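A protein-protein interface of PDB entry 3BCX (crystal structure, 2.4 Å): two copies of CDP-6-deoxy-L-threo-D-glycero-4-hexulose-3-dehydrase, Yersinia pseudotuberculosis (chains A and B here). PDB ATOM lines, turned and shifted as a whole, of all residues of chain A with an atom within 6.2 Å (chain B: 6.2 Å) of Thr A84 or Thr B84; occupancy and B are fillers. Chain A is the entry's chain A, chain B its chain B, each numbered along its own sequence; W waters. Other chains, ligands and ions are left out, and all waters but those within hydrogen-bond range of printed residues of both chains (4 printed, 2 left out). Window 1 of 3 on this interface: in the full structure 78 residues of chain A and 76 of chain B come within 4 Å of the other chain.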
ATOM      1  N   THR A  82      28.570 -31.437 -15.191  1.00  0.00           N
ATOM      2  CA  THR A  82      28.123 -30.052 -15.198  1.00  0.00           C
ATOM      3  C   THR A  82      27.081 -29.845 -16.295  1.00  0.00           C
ATOM      4  O   THR A  82      27.101 -30.526 -17.322  1.00  0.00           O
ATOM      5  CB  THR A  82      29.279 -29.047 -15.435  1.00  0.00           C
ATOM      6  OG1 THR A  82      29.983 -29.383 -16.637  1.00  0.00           O
ATOM      7  CG2 THR A  82      30.236 -29.036 -14.252  1.00  0.00           C
ATOM      8  N   THR A  83      26.164 -28.915 -16.057  1.00  0.00           N
ATOM      9  CA  THR A  83      25.113 -28.598 -17.019  1.00  0.00           C
ATOM     10  C   THR A  83      24.842 -27.087 -16.920  1.00  0.00           C
ATOM     11  O   THR A  83      25.449 -26.417 -16.087  1.00  0.00           O
ATOM     12  CB  THR A  83      23.837 -29.450 -16.749  1.00  0.00           C
ATOM     13  OG1 THR A  83      22.863 -29.174 -17.760  1.00  0.00           O
ATOM     14  CG2 THR A  83      23.257 -29.162 -15.361  1.00  0.00           C
ATOM     15  N   THR A  84      23.934 -26.555 -17.740  1.00  0.00           N
ATOM     16  CA  THR A  84      23.680 -25.111 -17.776  1.00  0.00           C
ATOM     17  C   THR A  84      23.046 -24.412 -16.578  1.00  0.00           C
ATOM     18  O   THR A  84      23.161 -23.189 -16.446  1.00  0.00           O
ATOM     19  CB  THR A  84      22.830 -24.724 -19.001  1.00  0.00           C
ATOM     20  OG1 THR A  84      21.457 -25.065 -18.757  1.00  0.00           O
ATOM     21  CG2 THR A  84      23.323 -25.444 -20.248  1.00  0.00           C
ATOM     22  N   SER A  85      22.381 -25.158 -15.704  1.00  0.00           N
ATOM     23  CA  SER A  85      21.747 -24.523 -14.558  1.00  0.00           C
ATOM     24  C   SER A  85      21.192 -25.562 -13.610  1.00  0.00           C
ATOM     25  O   SER A  85      21.209 -26.753 -13.907  1.00  0.00           O
ATOM     26  CB  SER A  85      20.594 -23.629 -15.033  1.00  0.00           C
ATOM     27  OG  SER A  85      19.573 -24.417 -15.648  1.00  0.00           O
ATOM     28  N   GLY A  86      20.692 -25.104 -12.468  1.00  0.00           N
ATOM     29  CA  GLY A  86      20.104 -26.016 -11.511  1.00  0.00           C
ATOM     30  C   GLY A  86      18.902 -26.682 -12.147  1.00  0.00           C
ATOM     31  O   GLY A  86      18.669 -27.888 -11.960  1.00  0.00           O
ATOM     32  N   SER A  88      18.362 -27.186 -15.369  1.00  0.00           N
ATOM     33  CA  SER A  88      18.792 -28.155 -16.360  1.00  0.00           C
ATOM     34  C   SER A  88      19.238 -29.425 -15.643  1.00  0.00           C
ATOM     35  O   SER A  88      19.041 -30.538 -16.155  1.00  0.00           O
ATOM     36  CB  SER A  88      19.925 -27.576 -17.202  1.00  0.00           C
ATOM     37  OG  SER A  88      19.419 -26.532 -18.007  1.00  0.00           O
ATOM     38  N   ALA A  89      19.821 -29.260 -14.456  1.00  0.00           N
ATOM     39  CA  ALA A  89      20.257 -30.413 -13.680  1.00  0.00           C
ATOM     40  C   ALA A  89      19.036 -31.269 -13.310  1.00  0.00           C
ATOM     41  O   ALA A  89      19.031 -32.484 -13.522  1.00  0.00           O
ATOM     42  CB  ALA A  89      20.997 -29.958 -12.420  1.00  0.00           C
ATOM     43  N   GLU A 226      25.880 -18.786 -14.529  1.00  0.00           N
ATOM     44  CA  GLU A 226      24.800 -19.683 -14.904  1.00  0.00           C
ATOM     45  C   GLU A 226      25.483 -21.044 -14.942  1.00  0.00           C
ATOM     46  O   GLU A 226      26.551 -21.194 -15.539  1.00  0.00           O
ATOM     47  CB  GLU A 226      24.225 -19.342 -16.289  1.00  0.00           C
ATOM     48  CG  GLU A 226      23.456 -18.017 -16.380  1.00  0.00           C
ATOM     49  CD  GLU A 226      22.073 -18.039 -15.698  1.00  0.00           C
ATOM     50  OE1 GLU A 226      21.634 -19.109 -15.212  1.00  0.00           O
ATOM     51  OE2 GLU A 226      21.421 -16.973 -15.659  1.00  0.00           O
ATOM     52  N   GLY A 227      24.885 -22.028 -14.282  1.00  0.00           N
ATOM     53  CA  GLY A 227      25.471 -23.350 -14.287  1.00  0.00           C
ATOM     54  C   GLY A 227      24.870 -24.219 -13.210  1.00  0.00           C
ATOM     55  O   GLY A 227      24.187 -23.738 -12.314  1.00  0.00           O
ATOM     56  N   GLY A 228      25.131 -25.512 -13.300  1.00  0.00           N
ATOM     57  CA  GLY A 228      24.612 -26.436 -12.318  1.00  0.00           C
ATOM     58  C   GLY A 228      25.291 -27.762 -12.536  1.00  0.00           C
ATOM     59  O   GLY A 228      26.116 -27.900 -13.449  1.00  0.00           O
ATOM     60  N   ASN A 288      21.049 -30.375 -25.569  1.00  0.00           N
ATOM     61  CA  ASN A 288      22.448 -29.995 -25.506  1.00  0.00           C
ATOM     62  C   ASN A 288      22.468 -28.999 -24.354  1.00  0.00           C
ATOM     63  O   ASN A 288      22.137 -27.826 -24.518  1.00  0.00           O
ATOM     64  CB  ASN A 288      22.966 -29.323 -26.773  1.00  0.00           C
ATOM     65  CG  ASN A 288      24.447 -28.966 -26.648  1.00  0.00           C
ATOM     66  OD1 ASN A 288      25.039 -28.330 -27.523  1.00  0.00           O
ATOM     67  ND2 ASN A 288      25.049 -29.378 -25.535  1.00  0.00           N
ATOM     68  N   LEU A 289      22.830 -29.489 -23.174  1.00  0.00           N
ATOM     69  CA  LEU A 289      22.858 -28.662 -21.982  1.00  0.00           C
ATOM     70  C   LEU A 289      24.245 -28.635 -21.336  1.00  0.00           C
ATOM     71  O   LEU A 289      24.395 -28.889 -20.138  1.00  0.00           O
ATOM     72  CB  LEU A 289      21.802 -29.180 -20.999  1.00  0.00           C
ATOM     73  CG  LEU A 289      20.379 -29.172 -21.581  1.00  0.00           C
ATOM     74  CD1 LEU A 289      19.416 -29.910 -20.661  1.00  0.00           C
ATOM     75  CD2 LEU A 289      19.920 -27.728 -21.812  1.00  0.00           C
ATOM     76  N   LYS A 290      25.256 -28.325 -22.144  1.00  0.00           N
ATOM     77  CA  LYS A 290      26.637 -28.240 -21.668  1.00  0.00           C
ATOM     78  C   LYS A 290      27.022 -26.785 -21.369  1.00  0.00           C
ATOM     79  O   LYS A 290      26.310 -25.856 -21.757  1.00  0.00           O
ATOM     80  CB  LYS A 290      27.601 -28.827 -22.719  1.00  0.00           C
ATOM     81  CG  LYS A 290      27.527 -30.336 -22.857  1.00  0.00           C
ATOM     82  CD  LYS A 290      28.627 -30.875 -23.774  1.00  0.00           C
ATOM     83  CE  LYS A 290      28.140 -31.151 -25.198  1.00  0.00           C
ATOM     84  NZ  LYS A 290      27.809 -29.925 -25.969  1.00  0.00           N
ATOM     85  N   ILE A 291      28.137 -26.593 -20.668  1.00  0.00           N
ATOM     86  CA  ILE A 291      28.617 -25.243 -20.351  1.00  0.00           C
ATOM     87  C   ILE A 291      30.011 -25.026 -20.935  1.00  0.00           C
ATOM     88  O   ILE A 291      30.583 -25.925 -21.559  1.00  0.00           O
ATOM     89  CB  ILE A 291      28.705 -24.997 -18.829  1.00  0.00           C
ATOM     90  CG1 ILE A 291      29.717 -25.957 -18.200  1.00  0.00           C
ATOM     91  CG2 ILE A 291      27.327 -25.147 -18.193  1.00  0.00           C
ATOM     92  CD1 ILE A 291      29.969 -25.696 -16.728  1.00  0.00           C
ATOM     93  N   GLN A 295      32.922 -20.793 -17.585  1.00  0.00           N
ATOM     94  CA  GLN A 295      31.981 -20.970 -16.487  1.00  0.00           C
ATOM     95  C   GLN A 295      32.551 -21.924 -15.452  1.00  0.00           C
ATOM     96  O   GLN A 295      32.410 -21.702 -14.249  1.00  0.00           O
ATOM     97  CB  GLN A 295      30.658 -21.534 -17.008  1.00  0.00           C
ATOM     98  CG  GLN A 295      29.775 -20.538 -17.715  1.00  0.00           C
ATOM     99  CD  GLN A 295      28.734 -21.221 -18.579  1.00  0.00           C
ATOM    100  OE1 GLN A 295      29.032 -21.681 -19.684  1.00  0.00           O
ATOM    101  NE2 GLN A 295      27.508 -21.304 -18.075  1.00  0.00           N
ATOM    102  N   THR B  82      19.333 -14.881 -26.497  1.00  0.00           N
ATOM    103  CA  THR B  82      20.384 -15.876 -26.372  1.00  0.00           C
ATOM    104  C   THR B  82      19.953 -17.002 -25.432  1.00  0.00           C
ATOM    105  O   THR B  82      19.176 -16.794 -24.496  1.00  0.00           O
ATOM    106  CB  THR B  82      21.695 -15.273 -25.835  1.00  0.00           C
ATOM    107  OG1 THR B  82      21.465 -14.674 -24.556  1.00  0.00           O
ATOM    108  CG2 THR B  82      22.239 -14.235 -26.807  1.00  0.00           C
ATOM    109  N   THR B  83      20.465 -18.198 -25.705  1.00  0.00           N
ATOM    110  CA  THR B  83      20.179 -19.381 -24.906  1.00  0.00           C
ATOM    111  C   THR B  83      21.435 -20.263 -24.907  1.00  0.00           C
ATOM    112  O   THR B  83      22.407 -19.941 -25.582  1.00  0.00           O
ATOM    113  CB  THR B  83      18.934 -20.141 -25.454  1.00  0.00           C
ATOM    114  OG1 THR B  83      18.669 -21.270 -24.619  1.00  0.00           O
ATOM    115  CG2 THR B  83      19.145 -20.589 -26.900  1.00  0.00           C
ATOM    116  N   THR B  84      21.410 -21.373 -24.176  1.00  0.00           N
ATOM    117  CA  THR B  84      22.587 -22.230 -24.036  1.00  0.00           C
ATOM    118  C   THR B  84      23.139 -22.979 -25.247  1.00  0.00           C
ATOM    119  O   THR B  84      24.304 -23.387 -25.243  1.00  0.00           O
ATOM    120  CB  THR B  84      22.378 -23.277 -22.919  1.00  0.00           C
ATOM    121  OG1 THR B  84      21.593 -24.372 -23.418  1.00  0.00           O
ATOM    122  CG2 THR B  84      21.680 -22.634 -21.727  1.00  0.00           C
ATOM    123  N   SER B  85      22.324 -23.175 -26.275  1.00  0.00           N
ATOM    124  CA  SER B  85      22.806 -23.905 -27.435  1.00  0.00           C
ATOM    125  C   SER B  85      21.814 -23.825 -28.572  1.00  0.00           C
ATOM    126  O   SER B  85      20.705 -23.314 -28.409  1.00  0.00           O
ATOM    127  CB  SER B  85      23.025 -25.378 -27.070  1.00  0.00           C
ATOM    128  OG  SER B  85      21.789 -26.006 -26.731  1.00  0.00           O
ATOM    129  N   GLY B  86      22.220 -24.340 -29.726  1.00  0.00           N
ATOM    130  CA  GLY B  86      21.329 -24.346 -30.863  1.00  0.00           C
ATOM    131  C   GLY B  86      20.137 -25.215 -30.519  1.00  0.00           C
ATOM    132  O   GLY B  86      18.991 -24.905 -30.886  1.00  0.00           O
ATOM    133  N   SER B  88      18.916 -25.823 -27.506  1.00  0.00           N
ATOM    134  CA  SER B  88      18.041 -25.154 -26.563  1.00  0.00           C
ATOM    135  C   SER B  88      17.188 -24.130 -27.300  1.00  0.00           C
ATOM    136  O   SER B  88      16.025 -23.901 -26.939  1.00  0.00           O
ATOM    137  CB  SER B  88      18.859 -24.479 -25.465  1.00  0.00           C
ATOM    138  OG  SER B  88      19.480 -25.463 -24.659  1.00  0.00           O
ATOM    139  N   ALA B  89      17.764 -23.522 -28.338  1.00  0.00           N
ATOM    140  CA  ALA B  89      17.037 -22.537 -29.121  1.00  0.00           C
ATOM    141  C   ALA B  89      15.873 -23.235 -29.817  1.00  0.00           C
ATOM    142  O   ALA B  89      14.741 -22.741 -29.793  1.00  0.00           O
ATOM    143  CB  ALA B  89      17.965 -21.878 -30.146  1.00  0.00           C
ATOM    144  N   GLU B 226      29.734 -22.631 -26.219  1.00  0.00           N
ATOM    145  CA  GLU B 226      28.435 -23.265 -26.113  1.00  0.00           C
ATOM    146  C   GLU B 226      27.470 -22.094 -26.079  1.00  0.00           C
ATOM    147  O   GLU B 226      27.619 -21.189 -25.253  1.00  0.00           O
ATOM    148  CB  GLU B 226      28.311 -24.082 -24.822  1.00  0.00           C
ATOM    149  CG  GLU B 226      29.169 -25.342 -24.778  1.00  0.00           C
ATOM    150  CD  GLU B 226      28.625 -26.491 -25.637  1.00  0.00           C
ATOM    151  OE1 GLU B 226      27.542 -26.350 -26.255  1.00  0.00           O
ATOM    152  OE2 GLU B 226      29.292 -27.545 -25.681  1.00  0.00           O
ATOM    153  N   GLY B 227      26.502 -22.094 -26.990  1.00  0.00           N
ATOM    154  CA  GLY B 227      25.532 -21.022 -27.016  1.00  0.00           C
ATOM    155  C   GLY B 227      24.649 -21.101 -28.240  1.00  0.00           C
ATOM    156  O   GLY B 227      24.912 -21.862 -29.162  1.00  0.00           O
ATOM    157  N   GLY B 228      23.589 -20.310 -28.243  1.00  0.00           N
ATOM    158  CA  GLY B 228      22.682 -20.294 -29.368  1.00  0.00           C
ATOM    159  C   GLY B 228      21.767 -19.110 -29.204  1.00  0.00           C
ATOM    160  O   GLY B 228      21.869 -18.378 -28.217  1.00  0.00           O
ATOM    161  N   ASN B 288      15.509 -23.155 -17.417  1.00  0.00           N
ATOM    162  CA  ASN B 288      16.442 -22.059 -17.217  1.00  0.00           C
ATOM    163  C   ASN B 288      17.535 -22.352 -18.238  1.00  0.00           C
ATOM    164  O   ASN B 288      18.418 -23.174 -18.008  1.00  0.00           O
ATOM    165  CB  ASN B 288      17.052 -21.994 -15.819  1.00  0.00           C
ATOM    166  CG  ASN B 288      18.004 -20.802 -15.680  1.00  0.00           C
ATOM    167  OD1 ASN B 288      18.686 -20.633 -14.666  1.00  0.00           O
ATOM    168  ND2 ASN B 288      18.051 -19.969 -16.718  1.00  0.00           N
ATOM    169  N   LEU B 289      17.448 -21.687 -19.383  1.00  0.00           N
ATOM    170  CA  LEU B 289      18.396 -21.896 -20.463  1.00  0.00           C
ATOM    171  C   LEU B 289      19.113 -20.599 -20.850  1.00  0.00           C
ATOM    172  O   LEU B 289      19.139 -20.215 -22.024  1.00  0.00           O
ATOM    173  CB  LEU B 289      17.642 -22.493 -21.660  1.00  0.00           C
ATOM    174  CG  LEU B 289      16.903 -23.790 -21.285  1.00  0.00           C
ATOM    175  CD1 LEU B 289      15.960 -24.229 -22.405  1.00  0.00           C
ATOM    176  CD2 LEU B 289      17.925 -24.886 -20.953  1.00  0.00           C
ATOM    177  N   LYS B 290      19.701 -19.937 -19.855  1.00  0.00           N
ATOM    178  CA  LYS B 290      20.422 -18.681 -20.074  1.00  0.00           C
ATOM    179  C   LYS B 290      21.940 -18.887 -20.129  1.00  0.00           C
ATOM    180  O   LYS B 290      22.449 -19.925 -19.708  1.00  0.00           O
ATOM    181  CB  LYS B 290      20.064 -17.666 -18.968  1.00  0.00           C
ATOM    182  CG  LYS B 290      18.662 -17.089 -19.102  1.00  0.00           C
ATOM    183  CD  LYS B 290      18.403 -15.960 -18.105  1.00  0.00           C
ATOM    184  CE  LYS B 290      17.769 -16.440 -16.800  1.00  0.00           C
ATOM    185  NZ  LYS B 290      18.650 -17.313 -15.973  1.00  0.00           N
ATOM    186  N   ILE B 291      22.659 -17.898 -20.655  1.00  0.00           N
ATOM    187  CA  ILE B 291      24.119 -17.988 -20.740  1.00  0.00           C
ATOM    188  C   ILE B 291      24.777 -16.918 -19.871  1.00  0.00           C
ATOM    189  O   ILE B 291      24.092 -16.104 -19.244  1.00  0.00           O
ATOM    190  CB  ILE B 291      24.630 -17.795 -22.189  1.00  0.00           C
ATOM    191  CG1 ILE B 291      24.250 -16.400 -22.692  1.00  0.00           C
ATOM    192  CG2 ILE B 291      24.072 -18.889 -23.095  1.00  0.00           C
ATOM    193  CD1 ILE B 291      24.898 -16.027 -24.007  1.00  0.00           C
ATOM    194  N   GLN B 295      30.273 -15.810 -22.337  1.00  0.00           N
ATOM    195  CA  GLN B 295      29.910 -16.450 -23.596  1.00  0.00           C
ATOM    196  C   GLN B 295      29.474 -15.395 -24.597  1.00  0.00           C
ATOM    197  O   GLN B 295      29.856 -15.443 -25.770  1.00  0.00           O
ATOM    198  CB  GLN B 295      28.763 -17.448 -23.378  1.00  0.00           C
ATOM    199  CG  GLN B 295      29.183 -18.761 -22.753  1.00  0.00           C
ATOM    200  CD  GLN B 295      28.023 -19.492 -22.093  1.00  0.00           C
ATOM    201  OE1 GLN B 295      27.551 -19.097 -21.028  1.00  0.00           O
ATOM    202  NE2 GLN B 295      27.560 -20.565 -22.727  1.00  0.00           N
HETATM  203  O   HOH W   1      16.459 -25.687 -18.002  1.00  0.00           O
HETATM  204  O   HOH W   2      18.906 -28.548 -25.126  1.00  0.00           O
HETATM  205  O   HOH W   3      22.105 -14.981 -17.208  1.00  0.00           O
HETATM  206  O   HOH W   4      31.259 -27.869 -23.899  1.00  0.00           O
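NZ of Lys B290 lies within salt-bridge range of OE2 of Glu A226, at 2.8 Å. The side-chain amide oxygen (OD1) of Asn A288 sits close to the side-chain carboxylate (OE1) of Glu B226 (3.4 Å). The backbone carbonyl oxygen (O) of Asn A288 lies within hydrogen-bond range of the side-chain hydroxyl (OG) of Ser B85. OG of Ser A85 lies within hydrogen-bond range of O of Asn B288 (2.9 Å). The side-chain amide oxygen (OD1) of Asn B288 sits close to the side-chain carboxylate (OE1) of Glu A226, 3.4 Å away. The side-chain amino group of Lys A290 lies within salt-bridge range of the side-chain carboxylate of Glu B226. The side-chain amide oxygen (OE1) of Gln A295 sits close to the side-chain amide oxygen (OE1) of Gln B295.
OG1 of Thr A84 sits at hydrogen-bond distance from OG of Ser A88 (2.6 Å). The backbone carbonyl oxygen (O) of Leu B289 is in hydrogen-bond range of the side-chain hydroxyl (OG1) of Thr B83. ND2 of Asn A288 lies close to NZ of Lys A290 (2.8 Å). O of Glu A226 sits at hydrogen-bond distance from NE2 of Gln A295, at 2.7 Å. O of Glu B226 is in hydrogen-bond range of NE2 of Gln B295 (2.6 Å). OG of Ser A85 sits at hydrogen-bond distance from N of Ser A88 (3.0 Å).
Thr B84 touches Thr A84. Thr A84 touches Asn B288. O of Asn B288 touches OG of Ser A88 (3.5 Å). Ser A88 touches Leu B289 (OG to CD2, 3.7 Å). Ile B291 touches Glu A226 (O to CG, 3.5 Å). O of Asn A288 touches OG1 of Thr B84 (3.7 Å). Asn A288 touches Ser B88 (O to OG, 3.6 Å). Ser B88 touches Leu A289 (OG to CD2, 3.7 Å). Leu B289 touches Leu A289 (CD2 to CD2, 3.6 Å). Ile A291 touches Glu B226.
Thr A84 touches just these residues of chain B: Thr B84 and Asn B288. Printed residues of chain B within 4 Å of Ser A88: Asn B288 and Leu B289. Gly A228 touches none of the printed residues of chain B. Of the printed residues of chain B, Ile A291 touches Glu B226. Of the printed residues of chain B, Gln A295 touches Gln B295 (3.3 Å). Of the printed residues of chain A, Thr B84 touches Thr A84 and Asn A288. Gly B86 touches none of the printed residues of chain A. The nearest residue of chain B that does not touch Thr A84 is Leu B289 (4.2 Å). The nearest printed residue of chain A that does not touch Ser B88 is Thr A84 (5.9 Å).
Hydrophobic or aromatic side chains of chain B that line the printed part of chain A: Leu B289. Among the printed residues, 17 pairs touch across the chains. Among the printed residues, Asp or Glu carboxylates within 4 Å of a Lys or Arg side-chain nitrogen of the other chain: Glu A226 with Lys B290 (2.8 Å) and Lys A290 with Glu B226 (2.8 Å).
Ser A88 touches Asn B288, and with the chains exchanged Asn A288 touches Ser B88. Glu A226 touches Lys B290, and with the chains exchanged Lys A290 touches Glu B226. Leu A289 touches its own counterpart, Leu B289. Gln B295 touches its own counterpart, Gln A295. 15 positions are printed for both chains.
Water W3 bridges the side-chain carboxylate (OE2) of Glu A226 and the backbone carbonyl oxygen (O) of Ile B291. Water W4 bridges the side-chain carboxylate of Glu B226 (2.7 Å) and the backbone carbonyl oxygen of Ile A291 (3.1 Å). Water W1 bridges the backbone NH (N) of Asn B288 (2.8 Å) and the side-chain hydroxyl (OG) of Ser A88 (3.1 Å). Water W2 lies within hydrogen-bond range of N of Asn A288 (2.9 Å) and OG of Ser B88 (3.2 Å).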
